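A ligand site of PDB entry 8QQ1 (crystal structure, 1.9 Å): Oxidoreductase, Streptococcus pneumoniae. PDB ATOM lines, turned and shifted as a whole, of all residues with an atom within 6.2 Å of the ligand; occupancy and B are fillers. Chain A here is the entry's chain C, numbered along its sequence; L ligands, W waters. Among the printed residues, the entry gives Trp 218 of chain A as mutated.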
ATOM      1  N   PHE A  39      11.748 -31.956  23.214  1.00  0.00           N
ATOM      2  CA  PHE A  39      11.917 -30.768  22.406  1.00  0.00           C
ATOM      3  C   PHE A  39      11.039 -29.630  22.937  1.00  0.00           C
ATOM      4  O   PHE A  39      10.187 -29.856  23.805  1.00  0.00           O
ATOM      5  CB  PHE A  39      11.580 -31.099  20.924  1.00  0.00           C
ATOM      6  CG  PHE A  39      10.134 -31.480  20.604  1.00  0.00           C
ATOM      7  CD1 PHE A  39       9.700 -32.794  20.752  1.00  0.00           C
ATOM      8  CD2 PHE A  39       9.240 -30.551  20.095  1.00  0.00           C
ATOM      9  CE1 PHE A  39       8.390 -33.162  20.428  1.00  0.00           C
ATOM     10  CE2 PHE A  39       7.918 -30.909  19.797  1.00  0.00           C
ATOM     11  CZ  PHE A  39       7.513 -32.216  19.955  1.00  0.00           C
ATOM     12  N   PHE A  41       9.217 -25.568  21.500  1.00  0.00           N
ATOM     13  CA  PHE A  41       8.927 -24.660  20.404  1.00  0.00           C
ATOM     14  C   PHE A  41       9.553 -23.320  20.749  1.00  0.00           C
ATOM     15  O   PHE A  41       9.231 -22.719  21.786  1.00  0.00           O
ATOM     16  CB  PHE A  41       7.415 -24.519  20.207  1.00  0.00           C
ATOM     17  CG  PHE A  41       6.802 -25.766  19.587  1.00  0.00           C
ATOM     18  CD1 PHE A  41       6.295 -26.779  20.386  1.00  0.00           C
ATOM     19  CD2 PHE A  41       6.681 -25.883  18.219  1.00  0.00           C
ATOM     20  CE1 PHE A  41       5.678 -27.901  19.819  1.00  0.00           C
ATOM     21  CE2 PHE A  41       6.052 -26.992  17.654  1.00  0.00           C
ATOM     22  CZ  PHE A  41       5.580 -28.014  18.448  1.00  0.00           C
ATOM     23  N   GLU A  50      11.439 -14.146  11.580  1.00  0.00           N
ATOM     24  CA  GLU A  50      10.033 -14.469  11.823  1.00  0.00           C
ATOM     25  C   GLU A  50       9.940 -14.954  13.303  1.00  0.00           C
ATOM     26  O   GLU A  50      10.880 -15.563  13.808  1.00  0.00           O
ATOM     27  CB  GLU A  50       9.494 -15.486  10.818  1.00  0.00           C
ATOM     28  CG  GLU A  50       9.836 -16.938  11.084  1.00  0.00           C
ATOM     29  CD  GLU A  50       9.387 -17.895   9.990  1.00  0.00           C
ATOM     30  OE1 GLU A  50       9.434 -19.121  10.234  1.00  0.00           O
ATOM     31  OE2 GLU A  50       9.003 -17.427   8.889  1.00  0.00           O
ATOM     32  N   PRO A  53       6.754 -19.961  15.976  1.00  0.00           N
ATOM     33  CA  PRO A  53       7.497 -20.987  16.724  1.00  0.00           C
ATOM     34  C   PRO A  53       7.998 -22.106  15.822  1.00  0.00           C
ATOM     35  O   PRO A  53       7.317 -22.498  14.877  1.00  0.00           O
ATOM     36  CB  PRO A  53       6.465 -21.530  17.721  1.00  0.00           C
ATOM     37  CG  PRO A  53       5.123 -21.304  17.052  1.00  0.00           C
ATOM     38  CD  PRO A  53       5.290 -20.039  16.212  1.00  0.00           C
ATOM     39  N   HIS A  54       9.147 -22.668  16.168  1.00  0.00           N
ATOM     40  CA  HIS A  54       9.726 -23.789  15.452  1.00  0.00           C
ATOM     41  C   HIS A  54      10.188 -24.773  16.525  1.00  0.00           C
ATOM     42  O   HIS A  54      10.825 -24.390  17.513  1.00  0.00           O
ATOM     43  CB  HIS A  54      10.941 -23.340  14.620  1.00  0.00           C
ATOM     44  CG  HIS A  54      10.597 -22.549  13.384  1.00  0.00           C
ATOM     45  ND1 HIS A  54      10.674 -23.114  12.120  1.00  0.00           N
ATOM     46  CD2 HIS A  54      10.221 -21.259  13.261  1.00  0.00           C
ATOM     47  CE1 HIS A  54      10.284 -22.166  11.290  1.00  0.00           C
ATOM     48  NE2 HIS A  54      10.006 -21.024  11.933  1.00  0.00           N
ATOM     49  N   PRO A  55       9.920 -26.067  16.297  1.00  0.00           N
ATOM     50  CA  PRO A  55      10.372 -27.070  17.269  1.00  0.00           C
ATOM     51  C   PRO A  55      11.841 -27.442  17.098  1.00  0.00           C
ATOM     52  O   PRO A  55      12.287 -27.696  15.988  1.00  0.00           O
ATOM     53  CB  PRO A  55       9.460 -28.273  16.965  1.00  0.00           C
ATOM     54  CG  PRO A  55       9.171 -28.164  15.492  1.00  0.00           C
ATOM     55  CD  PRO A  55       9.142 -26.676  15.175  1.00  0.00           C
ATOM     56  N   PHE A  56      12.580 -27.513  18.207  1.00  0.00           N
ATOM     57  CA  PHE A  56      13.965 -27.965  18.206  1.00  0.00           C
ATOM     58  C   PHE A  56      14.145 -28.837  19.449  1.00  0.00           C
ATOM     59  O   PHE A  56      13.672 -28.477  20.539  1.00  0.00           O
ATOM     60  CB  PHE A  56      14.977 -26.801  18.243  1.00  0.00           C
ATOM     61  CG  PHE A  56      14.898 -25.840  17.080  1.00  0.00           C
ATOM     62  CD1 PHE A  56      15.320 -26.222  15.813  1.00  0.00           C
ATOM     63  CD2 PHE A  56      14.363 -24.577  17.247  1.00  0.00           C
ATOM     64  CE1 PHE A  56      15.219 -25.348  14.733  1.00  0.00           C
ATOM     65  CE2 PHE A  56      14.268 -23.697  16.155  1.00  0.00           C
ATOM     66  CZ  PHE A  56      14.732 -24.079  14.918  1.00  0.00           C
ATOM     67  N   SER A  57      14.871 -29.955  19.296  1.00  0.00           N
ATOM     68  CA  SER A  57      15.183 -30.827  20.421  1.00  0.00           C
ATOM     69  C   SER A  57      16.079 -30.107  21.400  1.00  0.00           C
ATOM     70  O   SER A  57      16.940 -29.332  20.968  1.00  0.00           O
ATOM     71  CB  SER A  57      15.904 -32.084  19.950  1.00  0.00           C
ATOM     72  OG  SER A  57      15.119 -32.844  19.060  1.00  0.00           O
ATOM     73  N   ILE A  58      15.893 -30.314  22.716  1.00  0.00           N
ATOM     74  CA  ILE A  58      16.785 -29.701  23.689  1.00  0.00           C
ATOM     75  C   ILE A  58      18.150 -30.463  23.639  1.00  0.00           C
ATOM     76  O   ILE A  58      18.172 -31.694  23.746  1.00  0.00           O
ATOM     77  CB  ILE A  58      16.134 -29.607  25.075  1.00  0.00           C
ATOM     78  CG1 ILE A  58      14.856 -28.690  25.030  1.00  0.00           C
ATOM     79  CG2 ILE A  58      17.131 -29.103  26.114  1.00  0.00           C
ATOM     80  CD1 ILE A  58      13.694 -29.200  25.980  1.00  0.00           C
ATOM     81  N   PHE A  68      20.094 -25.386  22.288  1.00  0.00           N
ATOM     82  CA  PHE A  68      19.453 -25.927  21.095  1.00  0.00           C
ATOM     83  C   PHE A  68      20.536 -25.980  19.998  1.00  0.00           C
ATOM     84  O   PHE A  68      21.472 -25.172  20.005  1.00  0.00           O
ATOM     85  CB  PHE A  68      18.243 -25.088  20.635  1.00  0.00           C
ATOM     86  CG  PHE A  68      17.113 -25.061  21.616  1.00  0.00           C
ATOM     87  CD1 PHE A  68      16.164 -26.062  21.634  1.00  0.00           C
ATOM     88  CD2 PHE A  68      16.977 -24.011  22.509  1.00  0.00           C
ATOM     89  CE1 PHE A  68      15.093 -26.013  22.516  1.00  0.00           C
ATOM     90  CE2 PHE A  68      15.928 -23.986  23.434  1.00  0.00           C
ATOM     91  CZ  PHE A  68      14.986 -24.977  23.416  1.00  0.00           C
ATOM     92  N   THR A  69      20.467 -26.943  19.109  1.00  0.00           N
ATOM     93  CA  THR A  69      21.433 -27.071  18.037  1.00  0.00           C
ATOM     94  C   THR A  69      20.675 -27.107  16.741  1.00  0.00           C
ATOM     95  O   THR A  69      19.884 -28.004  16.508  1.00  0.00           O
ATOM     96  CB  THR A  69      22.361 -28.262  18.270  1.00  0.00           C
ATOM     97  OG1 THR A  69      22.889 -28.169  19.593  1.00  0.00           O
ATOM     98  CG2 THR A  69      23.492 -28.286  17.265  1.00  0.00           C
ATOM     99  N   VAL A  70      20.872 -26.069  15.947  1.00  0.00           N
ATOM    100  CA  VAL A  70      20.095 -25.876  14.726  1.00  0.00           C
ATOM    101  C   VAL A  70      20.883 -26.086  13.434  1.00  0.00           C
ATOM    102  O   VAL A  70      21.853 -25.363  13.188  1.00  0.00           O
ATOM    103  CB  VAL A  70      19.486 -24.462  14.742  1.00  0.00           C
ATOM    104  CG1 VAL A  70      18.659 -24.202  13.495  1.00  0.00           C
ATOM    105  CG2 VAL A  70      18.654 -24.226  16.015  1.00  0.00           C
ATOM    106  N   LYS A  71      20.404 -26.996  12.576  1.00  0.00           N
ATOM    107  CA  LYS A  71      20.990 -27.270  11.256  1.00  0.00           C
ATOM    108  C   LYS A  71      20.181 -26.500  10.186  1.00  0.00           C
ATOM    109  O   LYS A  71      18.950 -26.426  10.278  1.00  0.00           O
ATOM    110  CB  LYS A  71      20.944 -28.763  10.949  1.00  0.00           C
ATOM    111  CG  LYS A  71      21.542 -29.132   9.568  1.00  0.00           C
ATOM    112  CD  LYS A  71      20.858 -30.329   8.990  1.00  0.00           C
ATOM    113  CE  LYS A  71      21.361 -30.692   7.600  1.00  0.00           C
ATOM    114  NZ  LYS A  71      22.839 -30.877   7.556  1.00  0.00           N
ATOM    115  N   THR A  72      20.871 -25.892   9.198  1.00  0.00           N
ATOM    116  CA  THR A  72      20.217 -25.146   8.124  1.00  0.00           C
ATOM    117  C   THR A  72      19.389 -26.108   7.272  1.00  0.00           C
ATOM    118  O   THR A  72      19.921 -27.071   6.728  1.00  0.00           O
ATOM    119  CB  THR A  72      21.248 -24.437   7.247  1.00  0.00           C
ATOM    120  OG1 THR A  72      21.982 -23.506   8.035  1.00  0.00           O
ATOM    121  CG2 THR A  72      20.589 -23.713   6.063  1.00  0.00           C
ATOM    122  N   SER A  73      18.094 -25.872   7.190  1.00  0.00           N
ATOM    123  CA  SER A  73      17.148 -26.705   6.468  1.00  0.00           C
ATOM    124  C   SER A  73      16.138 -25.922   5.618  1.00  0.00           C
ATOM    125  O   SER A  73      15.353 -26.538   4.914  1.00  0.00           O
ATOM    126  CB  SER A  73      16.385 -27.594   7.430  1.00  0.00           C
ATOM    127  OG  SER A  73      17.303 -28.441   8.114  1.00  0.00           O
ATOM    128  N   GLY A  74      16.171 -24.609   5.712  1.00  0.00           N
ATOM    129  CA  GLY A  74      15.292 -23.691   5.005  1.00  0.00           C
ATOM    130  C   GLY A  74      15.590 -22.259   5.424  1.00  0.00           C
ATOM    131  O   GLY A  74      16.620 -21.995   6.050  1.00  0.00           O
ATOM    132  N   ASP A  75      14.678 -21.336   5.095  1.00  0.00           N
ATOM    133  CA  ASP A  75      14.840 -19.895   5.311  1.00  0.00           C
ATOM    134  C   ASP A  75      15.107 -19.460   6.768  1.00  0.00           C
ATOM    135  O   ASP A  75      16.045 -18.715   7.021  1.00  0.00           O
ATOM    136  CB  ASP A  75      13.631 -19.132   4.742  1.00  0.00           C
ATOM    137  CG  ASP A  75      13.544 -19.122   3.223  1.00  0.00           C
ATOM    138  OD1 ASP A  75      14.531 -19.532   2.565  1.00  0.00           O
ATOM    139  OD2 ASP A  75      12.494 -18.690   2.693  1.00  0.00           O
ATOM    140  N   HIS A  76      14.281 -19.913   7.714  1.00  0.00           N
ATOM    141  CA  HIS A  76      14.424 -19.506   9.103  1.00  0.00           C
ATOM    142  C   HIS A  76      15.701 -20.057   9.745  1.00  0.00           C
ATOM    143  O   HIS A  76      16.422 -19.313  10.439  1.00  0.00           O
ATOM    144  CB  HIS A  76      13.165 -19.882   9.898  1.00  0.00           C
ATOM    145  CG  HIS A  76      13.245 -19.533  11.364  1.00  0.00           C
ATOM    146  ND1 HIS A  76      13.349 -18.221  11.781  1.00  0.00           N
ATOM    147  CD2 HIS A  76      13.182 -20.339  12.450  1.00  0.00           C
ATOM    148  CE1 HIS A  76      13.350 -18.264  13.101  1.00  0.00           C
ATOM    149  NE2 HIS A  76      13.256 -19.515  13.549  1.00  0.00           N
ATOM    150  N   THR A  77      16.016 -21.341   9.501  1.00  0.00           N
ATOM    151  CA  THR A  77      17.204 -21.943  10.090  1.00  0.00           C
ATOM    152  C   THR A  77      18.488 -21.432   9.403  1.00  0.00           C
ATOM    153  O   THR A  77      19.535 -21.388  10.055  1.00  0.00           O
ATOM    154  CB  THR A  77      17.074 -23.459  10.174  1.00  0.00           C
ATOM    155  OG1 THR A  77      16.816 -24.007   8.872  1.00  0.00           O
ATOM    156  CG2 THR A  77      15.944 -23.885  11.139  1.00  0.00           C
ATOM    157  N   LYS A  78      18.419 -21.024   8.116  1.00  0.00           N
ATOM    158  CA  LYS A  78      19.584 -20.403   7.461  1.00  0.00           C
ATOM    159  C   LYS A  78      19.816 -19.014   8.112  1.00  0.00           C
ATOM    160  O   LYS A  78      20.955 -18.634   8.426  1.00  0.00           O
ATOM    161  CB  LYS A  78      19.382 -20.249   5.950  1.00  0.00           C
ATOM    162  CG  LYS A  78      20.565 -19.589   5.263  1.00  0.00           C
ATOM    163  CD  LYS A  78      20.368 -19.476   3.759  1.00  0.00           C
ATOM    164  CE  LYS A  78      21.551 -18.771   3.148  1.00  0.00           C
ATOM    165  NZ  LYS A  78      22.806 -19.541   3.379  1.00  0.00           N
ATOM    166  N   ILE A 115      21.610 -34.197  12.438  1.00  0.00           N
ATOM    167  CA  ILE A 115      21.195 -33.347  13.568  1.00  0.00           C
ATOM    168  C   ILE A 115      20.281 -34.110  14.588  1.00  0.00           C
ATOM    169  O   ILE A 115      20.027 -33.600  15.657  1.00  0.00           O
ATOM    170  CB  ILE A 115      20.560 -31.995  13.085  1.00  0.00           C
ATOM    171  CG1 ILE A 115      20.559 -30.919  14.190  1.00  0.00           C
ATOM    172  CG2 ILE A 115      19.161 -32.190  12.502  1.00  0.00           C
ATOM    173  CD1 ILE A 115      21.923 -30.567  14.707  1.00  0.00           C
ATOM    174  N   THR A 118      21.057 -34.398  18.523  1.00  0.00           N
ATOM    175  CA  THR A 118      20.790 -33.415  19.594  1.00  0.00           C
ATOM    176  C   THR A 118      20.152 -33.962  20.882  1.00  0.00           C
ATOM    177  O   THR A 118      20.726 -33.619  21.905  1.00  0.00           O
ATOM    178  CB  THR A 118      20.028 -32.226  19.051  1.00  0.00           C
ATOM    179  OG1 THR A 118      18.826 -32.675  18.435  1.00  0.00           O
ATOM    180  CG2 THR A 118      20.871 -31.476  18.040  1.00  0.00           C
ATOM    181  N   PRO A 119      19.071 -34.792  20.948  1.00  0.00           N
ATOM    182  CA  PRO A 119      18.614 -35.285  22.259  1.00  0.00           C
ATOM    183  C   PRO A 119      19.671 -36.142  22.974  1.00  0.00           C
ATOM    184  O   PRO A 119      19.734 -36.145  24.189  1.00  0.00           O
ATOM    185  CB  PRO A 119      17.350 -36.097  21.912  1.00  0.00           C
ATOM    186  CG  PRO A 119      17.564 -36.526  20.491  1.00  0.00           C
ATOM    187  CD  PRO A 119      18.193 -35.292  19.866  1.00  0.00           C
ATOM    188  N   GLU A 216      12.138 -40.549  17.539  1.00  0.00           N
ATOM    189  CA  GLU A 216      11.583 -39.234  17.235  1.00  0.00           C
ATOM    190  C   GLU A 216      12.188 -38.862  15.874  1.00  0.00           C
ATOM    191  O   GLU A 216      13.404 -38.751  15.748  1.00  0.00           O
ATOM    192  CB  GLU A 216      12.037 -38.233  18.302  1.00  0.00           C
ATOM    193  CG  GLU A 216      11.462 -36.844  18.122  1.00  0.00           C
ATOM    194  CD  GLU A 216      10.006 -36.764  18.531  1.00  0.00           C
ATOM    195  OE1 GLU A 216       9.730 -36.854  19.749  1.00  0.00           O
ATOM    196  OE2 GLU A 216       9.144 -36.615  17.627  1.00  0.00           O
ATOM    197  N   GLY A 217      11.353 -38.709  14.864  1.00  0.00           N
ATOM    198  CA  GLY A 217      11.842 -38.344  13.538  1.00  0.00           C
ATOM    199  C   GLY A 217      11.220 -37.061  13.018  1.00  0.00           C
ATOM    200  O   GLY A 217      10.122 -36.691  13.434  1.00  0.00           O
ATOM    201  N   TRP A 218      11.939 -36.359  12.146  1.00  0.00           N
ATOM    202  CA  TRP A 218      11.371 -35.159  11.498  1.00  0.00           C
ATOM    203  C   TRP A 218      11.794 -35.079  10.035  1.00  0.00           C
ATOM    204  O   TRP A 218      12.834 -35.612   9.670  1.00  0.00           O
ATOM    205  CB  TRP A 218      11.653 -33.861  12.266  1.00  0.00           C
ATOM    206  CG  TRP A 218      13.096 -33.534  12.514  1.00  0.00           C
ATOM    207  CD1 TRP A 218      13.905 -32.776  11.717  1.00  0.00           C
ATOM    208  CD2 TRP A 218      13.849 -33.818  13.703  1.00  0.00           C
ATOM    209  NE1 TRP A 218      15.141 -32.618  12.313  1.00  0.00           N
ATOM    210  CE2 TRP A 218      15.123 -33.239  13.543  1.00  0.00           C
ATOM    211  CE3 TRP A 218      13.562 -34.494  14.883  1.00  0.00           C
ATOM    212  CZ2 TRP A 218      16.125 -33.356  14.507  1.00  0.00           C
ATOM    213  CZ3 TRP A 218      14.535 -34.555  15.870  1.00  0.00           C
ATOM    214  CH2 TRP A 218      15.793 -33.985  15.671  1.00  0.00           C
ATOM    215  N   LYS A 219      10.970 -34.450   9.189  1.00  0.00           N
ATOM    216  CA  LYS A 219      11.301 -34.307   7.765  1.00  0.00           C
ATOM    217  C   LYS A 219      12.477 -33.357   7.634  1.00  0.00           C
ATOM    218  O   LYS A 219      12.345 -32.181   7.966  1.00  0.00           O
ATOM    219  CB  LYS A 219      10.106 -33.755   6.971  1.00  0.00           C
ATOM    220  CG  LYS A 219       9.153 -34.819   6.467  1.00  0.00           C
ATOM    221  CD  LYS A 219       7.986 -34.177   5.743  1.00  0.00           C
ATOM    222  CE  LYS A 219       7.159 -35.177   4.977  1.00  0.00           C
ATOM    223  NZ  LYS A 219       6.128 -34.516   4.132  1.00  0.00           N
ATOM    224  N   PHE A 220      13.646 -33.864   7.234  1.00  0.00           N
ATOM    225  CA  PHE A 220      14.840 -33.039   7.091  1.00  0.00           C
ATOM    226  C   PHE A 220      14.697 -32.144   5.844  1.00  0.00           C
ATOM    227  O   PHE A 220      14.537 -32.664   4.738  1.00  0.00           O
ATOM    228  CB  PHE A 220      16.103 -33.911   6.960  1.00  0.00           C
ATOM    229  CG  PHE A 220      16.771 -34.233   8.278  1.00  0.00           C
ATOM    230  CD1 PHE A 220      16.028 -34.390   9.446  1.00  0.00           C
ATOM    231  CD2 PHE A 220      18.146 -34.412   8.361  1.00  0.00           C
ATOM    232  CE1 PHE A 220      16.640 -34.738  10.644  1.00  0.00           C
ATOM    233  CE2 PHE A 220      18.754 -34.756   9.569  1.00  0.00           C
ATOM    234  CZ  PHE A 220      17.994 -34.909  10.703  1.00  0.00           C
HETATM  235  P1  LIG L   1      11.100 -24.559   6.045  1.00  0.00           P
HETATM  236  O1  LIG L   1      11.236 -23.641   4.889  1.00  0.00           O
HETATM  237  O2  LIG L   1       9.878 -24.291   6.878  1.00  0.00           O
HETATM  238  O3  LIG L   1      11.207 -26.151   5.729  1.00  0.00           O
HETATM  239  C1  LIG L   1      10.013 -26.968   5.658  1.00  0.00           C
HETATM  240  C2  LIG L   1      10.252 -28.212   6.459  1.00  0.00           C
HETATM  241  O4  LIG L   1      10.780 -27.841   7.752  1.00  0.00           O
HETATM  242  C3  LIG L   1       9.008 -29.063   6.729  1.00  0.00           C
HETATM  243  O5  LIG L   1       8.868 -30.097   5.767  1.00  0.00           O
HETATM  244  C4  LIG L   1       9.265 -29.601   8.139  1.00  0.00           C
HETATM  245  O6  LIG L   1      10.074 -30.765   8.205  1.00  0.00           O
HETATM  246  C5  LIG L   1      10.035 -28.454   8.787  1.00  0.00           C
HETATM  247  N1  LIG L   1       9.203 -27.465   9.456  1.00  0.00           N
HETATM  248  C6  LIG L   1       8.949 -26.174   9.073  1.00  0.00           C
HETATM  249  N2  LIG L   1       8.202 -25.501   9.918  1.00  0.00           N
HETATM  250  C7  LIG L   1       7.937 -26.416  10.923  1.00  0.00           C
HETATM  251  C8  LIG L   1       7.131 -26.354  12.068  1.00  0.00           C
HETATM  252  N3  LIG L   1       6.479 -25.263  12.462  1.00  0.00           N
HETATM  253  N4  LIG L   1       6.991 -27.487  12.797  1.00  0.00           N
HETATM  254  C9  LIG L   1       7.646 -28.585  12.419  1.00  0.00           C
HETATM  255  N5  LIG L   1       8.453 -28.755  11.376  1.00  0.00           N
HETATM  256  C10 LIG L   1       8.545 -27.631  10.653  1.00  0.00           C
HETATM  257  N6  LIG L   1      15.941 -29.136  13.564  1.00  0.00           N
HETATM  258  C11 LIG L   1      17.199 -28.910  13.980  1.00  0.00           C
HETATM  259  O7  LIG L   1      17.995 -28.328  13.259  1.00  0.00           O
HETATM  260  N7  LIG L   1      17.602 -29.338  15.259  1.00  0.00           N
HETATM  261  C12 LIG L   1      16.808 -30.009  16.178  1.00  0.00           C
HETATM  262  O8  LIG L   1      17.257 -30.320  17.280  1.00  0.00           O
HETATM  263  C13 LIG L   1      15.430 -30.277  15.680  1.00  0.00           C
HETATM  264  N8  LIG L   1      14.616 -30.947  16.451  1.00  0.00           N
HETATM  265  C14 LIG L   1      13.299 -31.150  16.000  1.00  0.00           C
HETATM  266  C15 LIG L   1      12.397 -31.829  16.817  1.00  0.00           C
HETATM  267  C16 LIG L   1      11.089 -32.051  16.413  1.00  0.00           C
HETATM  268  C17 LIG L   1      10.190 -32.912  17.269  1.00  0.00           C
HETATM  269  C18 LIG L   1      10.657 -31.568  15.157  1.00  0.00           C
HETATM  270  C19 LIG L   1       9.243 -31.793  14.672  1.00  0.00           C
HETATM  271  C20 LIG L   1      11.556 -30.885  14.348  1.00  0.00           C
HETATM  272  C21 LIG L   1      12.874 -30.676  14.751  1.00  0.00           C
HETATM  273  N9  LIG L   1      13.811 -30.005  13.929  1.00  0.00           N
HETATM  274  C22 LIG L   1      15.105 -29.782  14.362  1.00  0.00           C
HETATM  275  C23 LIG L   1      13.428 -29.525  12.591  1.00  0.00           C
HETATM  276  C24 LIG L   1      13.110 -28.030  12.517  1.00  0.00           C
HETATM  277  O9  LIG L   1      11.958 -27.776  13.316  1.00  0.00           O
HETATM  278  C25 LIG L   1      12.932 -27.573  11.069  1.00  0.00           C
HETATM  279  O10 LIG L   1      14.124 -27.854  10.345  1.00  0.00           O
HETATM  280  C26 LIG L   1      12.684 -26.066  10.939  1.00  0.00           C
HETATM  281  O11 LIG L   1      11.540 -25.668  11.696  1.00  0.00           O
HETATM  282  C27 LIG L   1      12.528 -25.636   9.489  1.00  0.00           C
HETATM  283  O12 LIG L   1      12.341 -24.213   9.477  1.00  0.00           O
HETATM  284  P2  LIG L   1      12.819 -23.449   8.160  1.00  0.00           P
HETATM  285  O13 LIG L   1      12.097 -22.174   8.065  1.00  0.00           O
HETATM  286  O14 LIG L   1      14.330 -23.371   8.130  1.00  0.00           O
HETATM  287  O15 LIG L   1      12.390 -24.417   6.974  1.00  0.00           O
HETATM  288  O   HOH W   1       4.865 -28.038  14.479  1.00  0.00           O
HETATM  289  O   HOH W   2       5.983 -24.709  14.930  1.00  0.00           O
HETATM  290  O   HOH W   3       8.549 -32.956  10.447  1.00  0.00           O
HETATM  291  O   HOH W   4      16.525 -27.233  11.093  1.00  0.00           O
HETATM  292  O   HOH W   5      10.110 -30.845  11.196  1.00  0.00           O
HETATM  293  O   HOH W   6      13.751 -29.933   8.569  1.00  0.00           O
HETATM  294  O   HOH W   7      16.706 -30.622  10.574  1.00  0.00           O
HETATM  295  O   HOH W   8      18.442 -28.831  19.148  1.00  0.00           O
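A nitrogen (N9) of the ligand lies close to the indole nitrogen of Trp 218, at 3.3 Å.
CD1 of Phe 39 touches C17 of the ligand, at 3.5 Å.
Pro 53 touches the ligand.
Phe 56 touches the ligand (CA to N8, 3.5 Å).
Val 70 touches the ligand (CA to O7, 3.5 Å).
CB of Ser 73 touches O10 of the ligand, at 3.7 Å.
N of Asp 75 touches O14 of the ligand, 3.7 Å away.
Ile 115 touches the ligand.
OE2 of Glu 216 touches C17 of the ligand, at 3.9 Å.
Hydrophobic or aromatic side chains within 4 Å of the ligand: Phe 39, His 54, Pro 55, Phe 56, His 76, Ile 115 and Trp 218.
Within 4 Å of the ligand: Phe 39, Pro 53, His 54, Pro 55, Phe 56, Ser 57, Thr 69, Val 70, Lys 71, Ser 73, Gly 74, Asp 75, His 76, Thr 77, Ile 115, Thr 118, Glu 216, Trp 218 and Lys 219.
The nearest printed residue that does not touch the ligand is Glu 50 (4.6 Å).
The side-chain hydroxyl of Thr 77 sits at hydrogen-bond distance from the backbone NH of Gly 74.
OG1 of Thr 77 sits at hydrogen-bond distance from N of Ser 73, at 2.8 Å.
NE2 of His 54 lies within hydrogen-bond range of OE1 of Glu 50, at 2.6 Å.
OG of Ser 73 sits at hydrogen-bond distance from O of Lys 71, at 3.4 Å.
The side-chain hydroxyl (OG1) of Thr 118 is in hydrogen-bond range of the backbone carbonyl oxygen (O) of Ile 115, 3.2 Å away.
The backbone NH (N) of Thr 77 lies within hydrogen-bond range of an oxygen (O14) of the ligand (3.0 Å).
OG1 of Thr 77 sits at hydrogen-bond distance from O14 of the ligand (2.7 Å).
O6 of the ligand lies within hydrogen-bond range of O of Lys 219, 2.7 Å away.
O9 of the ligand sits at hydrogen-bond distance from O of Pro 55 (2.7 Å).
A ring nitrogen (ND1) of His 54 sits at hydrogen-bond distance from an oxygen (O11) of the ligand.
The backbone NH of Lys 71 is in hydrogen-bond range of an oxygen (O7) of the ligand (2.8 Å).
A nitrogen (N7) of the ligand is in hydrogen-bond range of the backbone carbonyl oxygen (O) of Thr 69 (2.9 Å).
N of Ser 57 is in hydrogen-bond range of N8 of the ligand (3.0 Å).
The side-chain hydroxyl of Ser 57 is in hydrogen-bond range of a nitrogen (N8) of the ligand (3.3 Å).
OG1 of Thr 118 sits at hydrogen-bond distance from O8 of the ligand, at 3.1 Å.
N of His 76 lies close to O13 of the ligand, 3.2 Å away.
O14 of the ligand lies close to N of Gly 74.
Water W2 bridges N3 of the ligand and O of Pro 53.
Water W4 lies within hydrogen-bond range of an oxygen (O10) of the ligand (2.6 Å), the backbone carbonyl oxygen of Lys 71 (2.7 Å) and the side-chain hydroxyl of Ser 73 (3.3 Å).
Water W8 lies within hydrogen-bond range of the backbone carbonyl oxygen (O) of Ser 57 (2.4 Å), an oxygen (O8) of the ligand (2.7 Å) and the backbone NH (N) of Thr 69 (2.8 Å).
Water W6 bridges O of Lys 219 and O10 of the ligand.
Water W7 lies within hydrogen-bond range of NE1 of Trp 218, OG of Ser 73 and N6 of the ligand.
Water W3 bridges the backbone NH (N) of Lys 219 and an oxygen (O6) of the ligand.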
